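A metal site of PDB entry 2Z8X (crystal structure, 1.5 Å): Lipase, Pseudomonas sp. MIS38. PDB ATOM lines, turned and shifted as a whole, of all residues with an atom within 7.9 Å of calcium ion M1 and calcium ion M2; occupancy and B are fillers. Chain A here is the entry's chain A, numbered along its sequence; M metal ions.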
ATOM      1  N   ALA A 343     -12.179  -0.752 -14.692  1.00  0.00           N
ATOM      2  CA  ALA A 343     -12.997  -1.324 -15.767  1.00  0.00           C
ATOM      3  C   ALA A 343     -12.223  -2.459 -16.418  1.00  0.00           C
ATOM      4  O   ALA A 343     -11.239  -2.221 -17.133  1.00  0.00           O
ATOM      5  CB  ALA A 343     -13.345  -0.246 -16.785  1.00  0.00           C
ATOM      6  N   ARG A 350     -18.689  -4.949 -22.051  1.00  0.00           N
ATOM      7  CA  ARG A 350     -18.419  -3.505 -22.031  1.00  0.00           C
ATOM      8  C   ARG A 350     -19.491  -2.722 -22.797  1.00  0.00           C
ATOM      9  O   ARG A 350     -19.826  -1.587 -22.428  1.00  0.00           O
ATOM     10  CB  ARG A 350     -17.029  -3.214 -22.600  1.00  0.00           C
ATOM     11  CG  ARG A 350     -16.614  -1.752 -22.502  1.00  0.00           C
ATOM     12  CD  ARG A 350     -15.225  -1.519 -23.093  1.00  0.00           C
ATOM     13  NE  ARG A 350     -15.143  -1.897 -24.498  1.00  0.00           N
ATOM     14  CZ  ARG A 350     -14.346  -2.839 -24.989  1.00  0.00           C
ATOM     15  NH1 ARG A 350     -13.507  -3.512 -24.206  1.00  0.00           N
ATOM     16  NH2 ARG A 350     -14.374  -3.089 -26.296  1.00  0.00           N
ATOM     17  N   ILE A 372     -11.921   3.942 -13.043  1.00  0.00           N
ATOM     18  CA  ILE A 372     -10.934   4.060 -14.112  1.00  0.00           C
ATOM     19  C   ILE A 372     -11.381   3.251 -15.328  1.00  0.00           C
ATOM     20  O   ILE A 372     -11.503   2.024 -15.266  1.00  0.00           O
ATOM     21  CB  ILE A 372      -9.527   3.591 -13.657  1.00  0.00           C
ATOM     22  CG1 ILE A 372      -9.129   4.194 -12.296  1.00  0.00           C
ATOM     23  CG2 ILE A 372      -8.476   3.892 -14.726  1.00  0.00           C
ATOM     24  CD1 ILE A 372      -9.158   5.722 -12.242  1.00  0.00           C
ATOM     25  N   GLY A 373     -11.621   3.952 -16.428  1.00  0.00           N
ATOM     26  CA  GLY A 373     -12.077   3.320 -17.658  1.00  0.00           C
ATOM     27  C   GLY A 373     -10.981   2.576 -18.419  1.00  0.00           C
ATOM     28  O   GLY A 373      -9.845   2.450 -17.951  1.00  0.00           O
ATOM     29  N   SER A 374     -11.367   2.090 -19.592  1.00  0.00           N
ATOM     30  CA  SER A 374     -10.464   1.411 -20.517  1.00  0.00           C
ATOM     31  C   SER A 374     -10.193   2.325 -21.704  1.00  0.00           C
ATOM     32  O   SER A 374     -10.802   3.385 -21.843  1.00  0.00           O
ATOM     33  CB  SER A 374     -11.109   0.104 -21.005  1.00  0.00           C
ATOM     34  OG  SER A 374     -12.123   0.375 -21.968  1.00  0.00           O
ATOM     35  N   ASP A 375      -9.280   1.904 -22.586  1.00  0.00           N
ATOM     36  CA  ASP A 375      -9.039   2.694 -23.797  1.00  0.00           C
ATOM     37  C   ASP A 375     -10.098   2.503 -24.887  1.00  0.00           C
ATOM     38  O   ASP A 375      -9.980   3.073 -25.973  1.00  0.00           O
ATOM     39  CB  ASP A 375      -7.624   2.468 -24.306  1.00  0.00           C
ATOM     40  CG  ASP A 375      -6.598   3.264 -23.490  1.00  0.00           C
ATOM     41  OD1 ASP A 375      -6.932   4.387 -23.027  1.00  0.00           O
ATOM     42  OD2 ASP A 375      -5.476   2.773 -23.342  1.00  0.00           O
ATOM     43  N   SER A 376     -11.134   1.729 -24.573  1.00  0.00           N
ATOM     44  CA  SER A 376     -12.261   1.553 -25.487  1.00  0.00           C
ATOM     45  C   SER A 376     -13.492   2.314 -24.991  1.00  0.00           C
ATOM     46  O   SER A 376     -13.418   3.054 -23.976  1.00  0.00           O
ATOM     47  CB  SER A 376     -12.545   0.069 -25.686  1.00  0.00           C
ATOM     48  OG  SER A 376     -11.420  -0.580 -26.265  1.00  0.00           O
ATOM     49  N   ASN A 377     -14.628   2.179 -25.686  1.00  0.00           N
ATOM     50  CA  ASN A 377     -15.865   2.881 -25.302  1.00  0.00           C
ATOM     51  C   ASN A 377     -16.462   2.298 -24.036  1.00  0.00           C
ATOM     52  O   ASN A 377     -16.885   1.136 -24.025  1.00  0.00           O
ATOM     53  CB  ASN A 377     -16.910   2.817 -26.425  1.00  0.00           C
ATOM     54  CG  ASN A 377     -16.417   3.405 -27.737  1.00  0.00           C
ATOM     55  OD1 ASN A 377     -15.327   3.953 -27.834  1.00  0.00           O
ATOM     56  ND2 ASN A 377     -17.254   3.293 -28.765  1.00  0.00           N
ATOM     57  N   ASP A 378     -16.477   3.090 -22.958  1.00  0.00           N
ATOM     58  CA  ASP A 378     -16.982   2.624 -21.667  1.00  0.00           C
ATOM     59  C   ASP A 378     -18.293   3.282 -21.295  1.00  0.00           C
ATOM     60  O   ASP A 378     -18.575   4.415 -21.700  1.00  0.00           O
ATOM     61  CB  ASP A 378     -15.988   2.941 -20.559  1.00  0.00           C
ATOM     62  CG  ASP A 378     -14.623   2.366 -20.809  1.00  0.00           C
ATOM     63  OD1 ASP A 378     -14.514   1.118 -20.962  1.00  0.00           O
ATOM     64  OD2 ASP A 378     -13.651   3.148 -20.823  1.00  0.00           O
ATOM     65  N   LEU A 379     -19.086   2.557 -20.502  1.00  0.00           N
ATOM     66  CA  LEU A 379     -20.241   3.082 -19.797  1.00  0.00           C
ATOM     67  C   LEU A 379     -19.859   3.117 -18.326  1.00  0.00           C
ATOM     68  O   LEU A 379     -19.638   2.074 -17.696  1.00  0.00           O
ATOM     69  CB  LEU A 379     -21.470   2.191 -20.015  1.00  0.00           C
ATOM     70  CG  LEU A 379     -21.912   1.878 -21.451  1.00  0.00           C
ATOM     71  CD1 LEU A 379     -23.077   0.910 -21.410  1.00  0.00           C
ATOM     72  CD2 LEU A 379     -22.284   3.142 -22.234  1.00  0.00           C
ATOM     73  N   ILE A 380     -19.747   4.328 -17.780  1.00  0.00           N
ATOM     74  CA  ILE A 380     -19.271   4.518 -16.400  1.00  0.00           C
ATOM     75  C   ILE A 380     -20.327   5.227 -15.553  1.00  0.00           C
ATOM     76  O   ILE A 380     -20.814   6.297 -15.917  1.00  0.00           O
ATOM     77  CB  ILE A 380     -17.965   5.326 -16.382  1.00  0.00           C
ATOM     78  CG1 ILE A 380     -16.833   4.512 -17.041  1.00  0.00           C
ATOM     79  CG2 ILE A 380     -17.598   5.738 -14.959  1.00  0.00           C
ATOM     80  CD1 ILE A 380     -15.628   5.341 -17.506  1.00  0.00           C
ATOM     81  N   GLU A 390     -12.887   8.508 -14.821  1.00  0.00           N
ATOM     82  CA  GLU A 390     -11.924   8.726 -15.893  1.00  0.00           C
ATOM     83  C   GLU A 390     -12.192   7.812 -17.087  1.00  0.00           C
ATOM     84  O   GLU A 390     -12.080   6.599 -16.994  1.00  0.00           O
ATOM     85  CB  GLU A 390     -10.496   8.508 -15.368  1.00  0.00           C
ATOM     86  CG  GLU A 390      -9.421   8.933 -16.355  1.00  0.00           C
ATOM     87  CD  GLU A 390      -8.013   8.762 -15.787  1.00  0.00           C
ATOM     88  OE1 GLU A 390      -7.794   7.751 -15.077  1.00  0.00           O
ATOM     89  OE2 GLU A 390      -7.154   9.630 -16.067  1.00  0.00           O
ATOM     90  N   GLY A 391     -12.552   8.404 -18.219  1.00  0.00           N
ATOM     91  CA  GLY A 391     -12.909   7.609 -19.398  1.00  0.00           C
ATOM     92  C   GLY A 391     -11.724   7.064 -20.188  1.00  0.00           C
ATOM     93  O   GLY A 391     -11.830   5.990 -20.801  1.00  0.00           O
ATOM     94  N   ARG A 392     -10.620   7.796 -20.184  1.00  0.00           N
ATOM     95  CA  ARG A 392      -9.472   7.493 -21.049  1.00  0.00           C
ATOM     96  C   ARG A 392      -9.914   7.539 -22.525  1.00  0.00           C
ATOM     97  O   ARG A 392     -10.902   8.199 -22.849  1.00  0.00           O
ATOM     98  CB  ARG A 392      -8.833   6.132 -20.685  1.00  0.00           C
ATOM     99  CG  ARG A 392      -8.263   6.051 -19.269  1.00  0.00           C
ATOM    100  CD  ARG A 392      -7.612   4.684 -18.991  1.00  0.00           C
ATOM    101  NE  ARG A 392      -6.593   4.332 -19.982  1.00  0.00           N
ATOM    102  CZ  ARG A 392      -5.275   4.506 -19.829  1.00  0.00           C
ATOM    103  NH1 ARG A 392      -4.788   5.048 -18.725  1.00  0.00           N
ATOM    104  NH2 ARG A 392      -4.452   4.137 -20.797  1.00  0.00           N
ATOM    105  N   ALA A 393      -9.201   6.844 -23.410  1.00  0.00           N
ATOM    106  CA  ALA A 393      -9.544   6.872 -24.838  1.00  0.00           C
ATOM    107  C   ALA A 393     -10.881   6.183 -25.076  1.00  0.00           C
ATOM    108  O   ALA A 393     -11.446   5.559 -24.181  1.00  0.00           O
ATOM    109  CB  ALA A 393      -8.453   6.222 -25.671  1.00  0.00           C
ATOM    110  N   GLY A 394     -11.395   6.306 -26.304  1.00  0.00           N
ATOM    111  CA  GLY A 394     -12.712   5.765 -26.608  1.00  0.00           C
ATOM    112  C   GLY A 394     -13.805   6.777 -26.326  1.00  0.00           C
ATOM    113  O   GLY A 394     -13.593   7.776 -25.595  1.00  0.00           O
ATOM    114  N   ASN A 395     -14.968   6.523 -26.903  1.00  0.00           N
ATOM    115  CA  ASN A 395     -16.144   7.366 -26.734  1.00  0.00           C
ATOM    116  C   ASN A 395     -16.896   6.875 -25.511  1.00  0.00           C
ATOM    117  O   ASN A 395     -17.583   5.854 -25.565  1.00  0.00           O
ATOM    118  CB  ASN A 395     -17.054   7.284 -27.965  1.00  0.00           C
ATOM    119  CG  ASN A 395     -16.385   7.829 -29.220  1.00  0.00           C
ATOM    120  OD1 ASN A 395     -15.330   8.471 -29.179  1.00  0.00           O
ATOM    121  ND2 ASN A 395     -17.008   7.555 -30.368  1.00  0.00           N
ATOM    122  N   ASP A 396     -16.726   7.592 -24.402  1.00  0.00           N
ATOM    123  CA  ASP A 396     -17.267   7.137 -23.123  1.00  0.00           C
ATOM    124  C   ASP A 396     -18.550   7.852 -22.753  1.00  0.00           C
ATOM    125  O   ASP A 396     -18.705   9.046 -23.051  1.00  0.00           O
ATOM    126  CB  ASP A 396     -16.217   7.338 -22.030  1.00  0.00           C
ATOM    127  CG  ASP A 396     -14.898   6.690 -22.381  1.00  0.00           C
ATOM    128  OD1 ASP A 396     -14.893   5.456 -22.575  1.00  0.00           O
ATOM    129  OD2 ASP A 396     -13.870   7.397 -22.476  1.00  0.00           O
ATOM    130  N   THR A 397     -19.461   7.122 -22.118  1.00  0.00           N
ATOM    131  CA  THR A 397     -20.680   7.703 -21.584  1.00  0.00           C
ATOM    132  C   THR A 397     -20.676   7.599 -20.072  1.00  0.00           C
ATOM    133  O   THR A 397     -20.410   6.525 -19.513  1.00  0.00           O
ATOM    134  CB  THR A 397     -21.937   7.034 -22.185  1.00  0.00           C
ATOM    135  OG1 THR A 397     -21.842   7.083 -23.610  1.00  0.00           O
ATOM    136  CG2 THR A 397     -23.211   7.767 -21.751  1.00  0.00           C
ATOM    137  N   PHE A 398     -20.941   8.716 -19.406  1.00  0.00           N
ATOM    138  CA  PHE A 398     -20.939   8.768 -17.952  1.00  0.00           C
ATOM    139  C   PHE A 398     -22.334   9.026 -17.402  1.00  0.00           C
ATOM    140  O   PHE A 398     -23.110   9.808 -17.993  1.00  0.00           O
ATOM    141  CB  PHE A 398     -20.032   9.909 -17.451  1.00  0.00           C
ATOM    142  CG  PHE A 398     -18.592   9.803 -17.891  1.00  0.00           C
ATOM    143  CD1 PHE A 398     -17.641   9.163 -17.086  1.00  0.00           C
ATOM    144  CD2 PHE A 398     -18.185  10.341 -19.110  1.00  0.00           C
ATOM    145  CE1 PHE A 398     -16.306   9.083 -17.511  1.00  0.00           C
ATOM    146  CE2 PHE A 398     -16.862  10.267 -19.523  1.00  0.00           C
ATOM    147  CZ  PHE A 398     -15.912   9.619 -18.724  1.00  0.00           C
ATOM    148  N   LEU A 408     -13.605  13.108 -16.227  1.00  0.00           N
ATOM    149  CA  LEU A 408     -12.631  13.369 -17.294  1.00  0.00           C
ATOM    150  C   LEU A 408     -12.921  12.485 -18.493  1.00  0.00           C
ATOM    151  O   LEU A 408     -12.695  11.272 -18.459  1.00  0.00           O
ATOM    152  CB  LEU A 408     -11.200  13.119 -16.811  1.00  0.00           C
ATOM    153  CG  LEU A 408     -10.707  13.971 -15.635  1.00  0.00           C
ATOM    154  CD1 LEU A 408      -9.299  13.560 -15.233  1.00  0.00           C
ATOM    155  CD2 LEU A 408     -10.761  15.465 -15.974  1.00  0.00           C
ATOM    156  N   GLY A 409     -13.426  13.097 -19.556  1.00  0.00           N
ATOM    157  CA  GLY A 409     -13.780  12.356 -20.764  1.00  0.00           C
ATOM    158  C   GLY A 409     -12.597  11.736 -21.474  1.00  0.00           C
ATOM    159  O   GLY A 409     -12.750  10.725 -22.160  1.00  0.00           O
ATOM    160  N   GLY A 410     -11.412  12.348 -21.352  1.00  0.00           N
ATOM    161  CA  GLY A 410     -10.227  11.910 -22.104  1.00  0.00           C
ATOM    162  C   GLY A 410     -10.398  12.084 -23.604  1.00  0.00           C
ATOM    163  O   GLY A 410     -11.262  12.849 -24.059  1.00  0.00           O
ATOM    164  N   ALA A 411      -9.586  11.363 -24.371  1.00  0.00           N
ATOM    165  CA  ALA A 411      -9.713  11.391 -25.836  1.00  0.00           C
ATOM    166  C   ALA A 411     -11.096  10.880 -26.253  1.00  0.00           C
ATOM    167  O   ALA A 411     -11.795  10.252 -25.460  1.00  0.00           O
ATOM    168  CB  ALA A 411      -8.615  10.547 -26.479  1.00  0.00           C
ATOM    169  N   GLY A 412     -11.493  11.165 -27.495  1.00  0.00           N
ATOM    170  CA  GLY A 412     -12.747  10.645 -28.031  1.00  0.00           C
ATOM    171  C   GLY A 412     -13.908  11.614 -27.931  1.00  0.00           C
ATOM    172  O   GLY A 412     -13.750  12.753 -27.467  1.00  0.00           O
ATOM    173  N   ASN A 413     -15.080  11.168 -28.375  1.00  0.00           N
ATOM    174  CA  ASN A 413     -16.307  11.946 -28.242  1.00  0.00           C
ATOM    175  C   ASN A 413     -17.070  11.412 -27.062  1.00  0.00           C
ATOM    176  O   ASN A 413     -17.636  10.315 -27.129  1.00  0.00           O
ATOM    177  CB  ASN A 413     -17.147  11.838 -29.519  1.00  0.00           C
ATOM    178  CG  ASN A 413     -16.467  12.483 -30.710  1.00  0.00           C
ATOM    179  OD1 ASN A 413     -15.974  13.619 -30.617  1.00  0.00           O
ATOM    180  ND2 ASN A 413     -16.444  11.779 -31.834  1.00  0.00           N
ATOM    181  N   ASN A 414     -17.081  12.168 -25.965  1.00  0.00           N
ATOM    182  CA  ASN A 414     -17.631  11.686 -24.717  1.00  0.00           C
ATOM    183  C   ASN A 414     -18.946  12.368 -24.345  1.00  0.00           C
ATOM    184  O   ASN A 414     -19.201  13.494 -24.780  1.00  0.00           O
ATOM    185  CB  ASN A 414     -16.601  11.877 -23.603  1.00  0.00           C
ATOM    186  CG  ASN A 414     -15.237  11.371 -24.000  1.00  0.00           C
ATOM    187  OD1 ASN A 414     -15.010  10.158 -24.116  1.00  0.00           O
ATOM    188  ND2 ASN A 414     -14.296  12.301 -24.205  1.00  0.00           N
ATOM    189  N   THR A 415     -19.745  11.680 -23.533  1.00  0.00           N
ATOM    190  CA  THR A 415     -21.092  12.105 -23.200  1.00  0.00           C
ATOM    191  C   THR A 415     -21.355  12.002 -21.699  1.00  0.00           C
ATOM    192  O   THR A 415     -20.972  11.012 -21.087  1.00  0.00           O
ATOM    193  CB  THR A 415     -22.148  11.235 -23.950  1.00  0.00           C
ATOM    194  OG1 THR A 415     -21.918  11.354 -25.358  1.00  0.00           O
ATOM    195  CG2 THR A 415     -23.580  11.668 -23.615  1.00  0.00           C
ATOM    196  N   ASP A 449     -13.471  17.587 -21.412  1.00  0.00           N
ATOM    197  CA  ASP A 449     -13.538  16.741 -22.598  1.00  0.00           C
ATOM    198  C   ASP A 449     -14.851  15.981 -22.728  1.00  0.00           C
ATOM    199  O   ASP A 449     -14.903  14.882 -23.293  1.00  0.00           O
ATOM    200  CB  ASP A 449     -12.327  15.792 -22.663  1.00  0.00           C
ATOM    201  CG  ASP A 449     -11.021  16.533 -22.709  1.00  0.00           C
ATOM    202  OD1 ASP A 449     -10.840  17.364 -23.637  1.00  0.00           O
ATOM    203  OD2 ASP A 449     -10.188  16.322 -21.808  1.00  0.00           O
ATOM    204  N   ILE A 450     -15.919  16.573 -22.218  1.00  0.00           N
ATOM    205  CA  ILE A 450     -17.251  16.033 -22.467  1.00  0.00           C
ATOM    206  C   ILE A 450     -17.984  17.027 -23.362  1.00  0.00           C
ATOM    207  O   ILE A 450     -18.300  18.137 -22.937  1.00  0.00           O
ATOM    208  CB  ILE A 450     -17.969  15.679 -21.148  1.00  0.00           C
ATOM    209  CG1 ILE A 450     -17.261  14.458 -20.508  1.00  0.00           C
ATOM    210  CG2 ILE A 450     -19.446  15.382 -21.397  1.00  0.00           C
ATOM    211  CD1 ILE A 450     -17.544  14.236 -19.060  1.00  0.00           C
HETATM  212 CA    CA M   1     -12.896   9.040 -23.772  1.00  0.00          CA
HETATM  213 CA    CA M   2     -12.680   4.612 -22.437  1.00  0.00          CA
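Six residues have an atom within 4 Å of calcium ion M2: Ser 374, Ser 376, Asp 378, Gly 391, Ala 393 and Asp 396.
Calcium ion M1 is bound by the side-chain carboxylate (OD2) of Asp 396 (2.3 Å), the backbone carbonyl oxygen (O) of Gly 394 (2.3 Å), the backbone carbonyl oxygen (O) of Gly 409 (2.3 Å), the backbone carbonyl oxygen (O) of Ala 411 (2.4 Å), the backbone carbonyl oxygen (O) of Arg 392 (2.4 Å) and the side-chain amide oxygen (OD1) of Asn 414 (2.4 Å).
The backbone carbonyl oxygen of Leu 408 is in hydrogen-bond range of the backbone NH of Gly 391 (2.9 Å). OG of Ser 374 lies close to N of Ser 376 (3.1 Å). The backbone NH (N) of Ala 393 is in hydrogen-bond range of the side-chain carboxylate (OD1) of Asp 375 (3.4 Å). The guanidinium group of Arg 392 lies within salt-bridge range of the side-chain carboxylate of Asp 375, at 3.1 Å. The backbone carbonyl oxygen (O) of Asp 378 lies within hydrogen-bond range of the backbone NH (N) of Thr 397 (2.9 Å). The side-chain amide nitrogen (ND2) of Asn 414 lies within hydrogen-bond range of the backbone carbonyl oxygen (O) of Gly 410, 3.1 Å away. The side-chain amide nitrogen (ND2) of Asn 414 is in hydrogen-bond range of the backbone carbonyl oxygen (O) of Gly 412 (3.3 Å). ND2 of Asn 414 sits at hydrogen-bond distance from O of Asp 449, at 2.8 Å.
Calcium ion M2 is bound by the backbone carbonyl oxygen of Gly 391, the backbone carbonyl oxygen of Ser 376, the backbone carbonyl oxygen of Ser 374, the backbone carbonyl oxygen of Ala 393, the side-chain carboxylate of Asp 396 and the side-chain carboxylate of Asp 378. Calcium ion M2 has six donor atoms within binding distance. Slightly farther from calcium ion M2 lies OD2 of Asp 396 (3.0 Å).
C of Gly 410 touches calcium ion M1 (3.9 Å). Of the 30 residues printed, 8 come within 4 Å of calcium ion M1.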
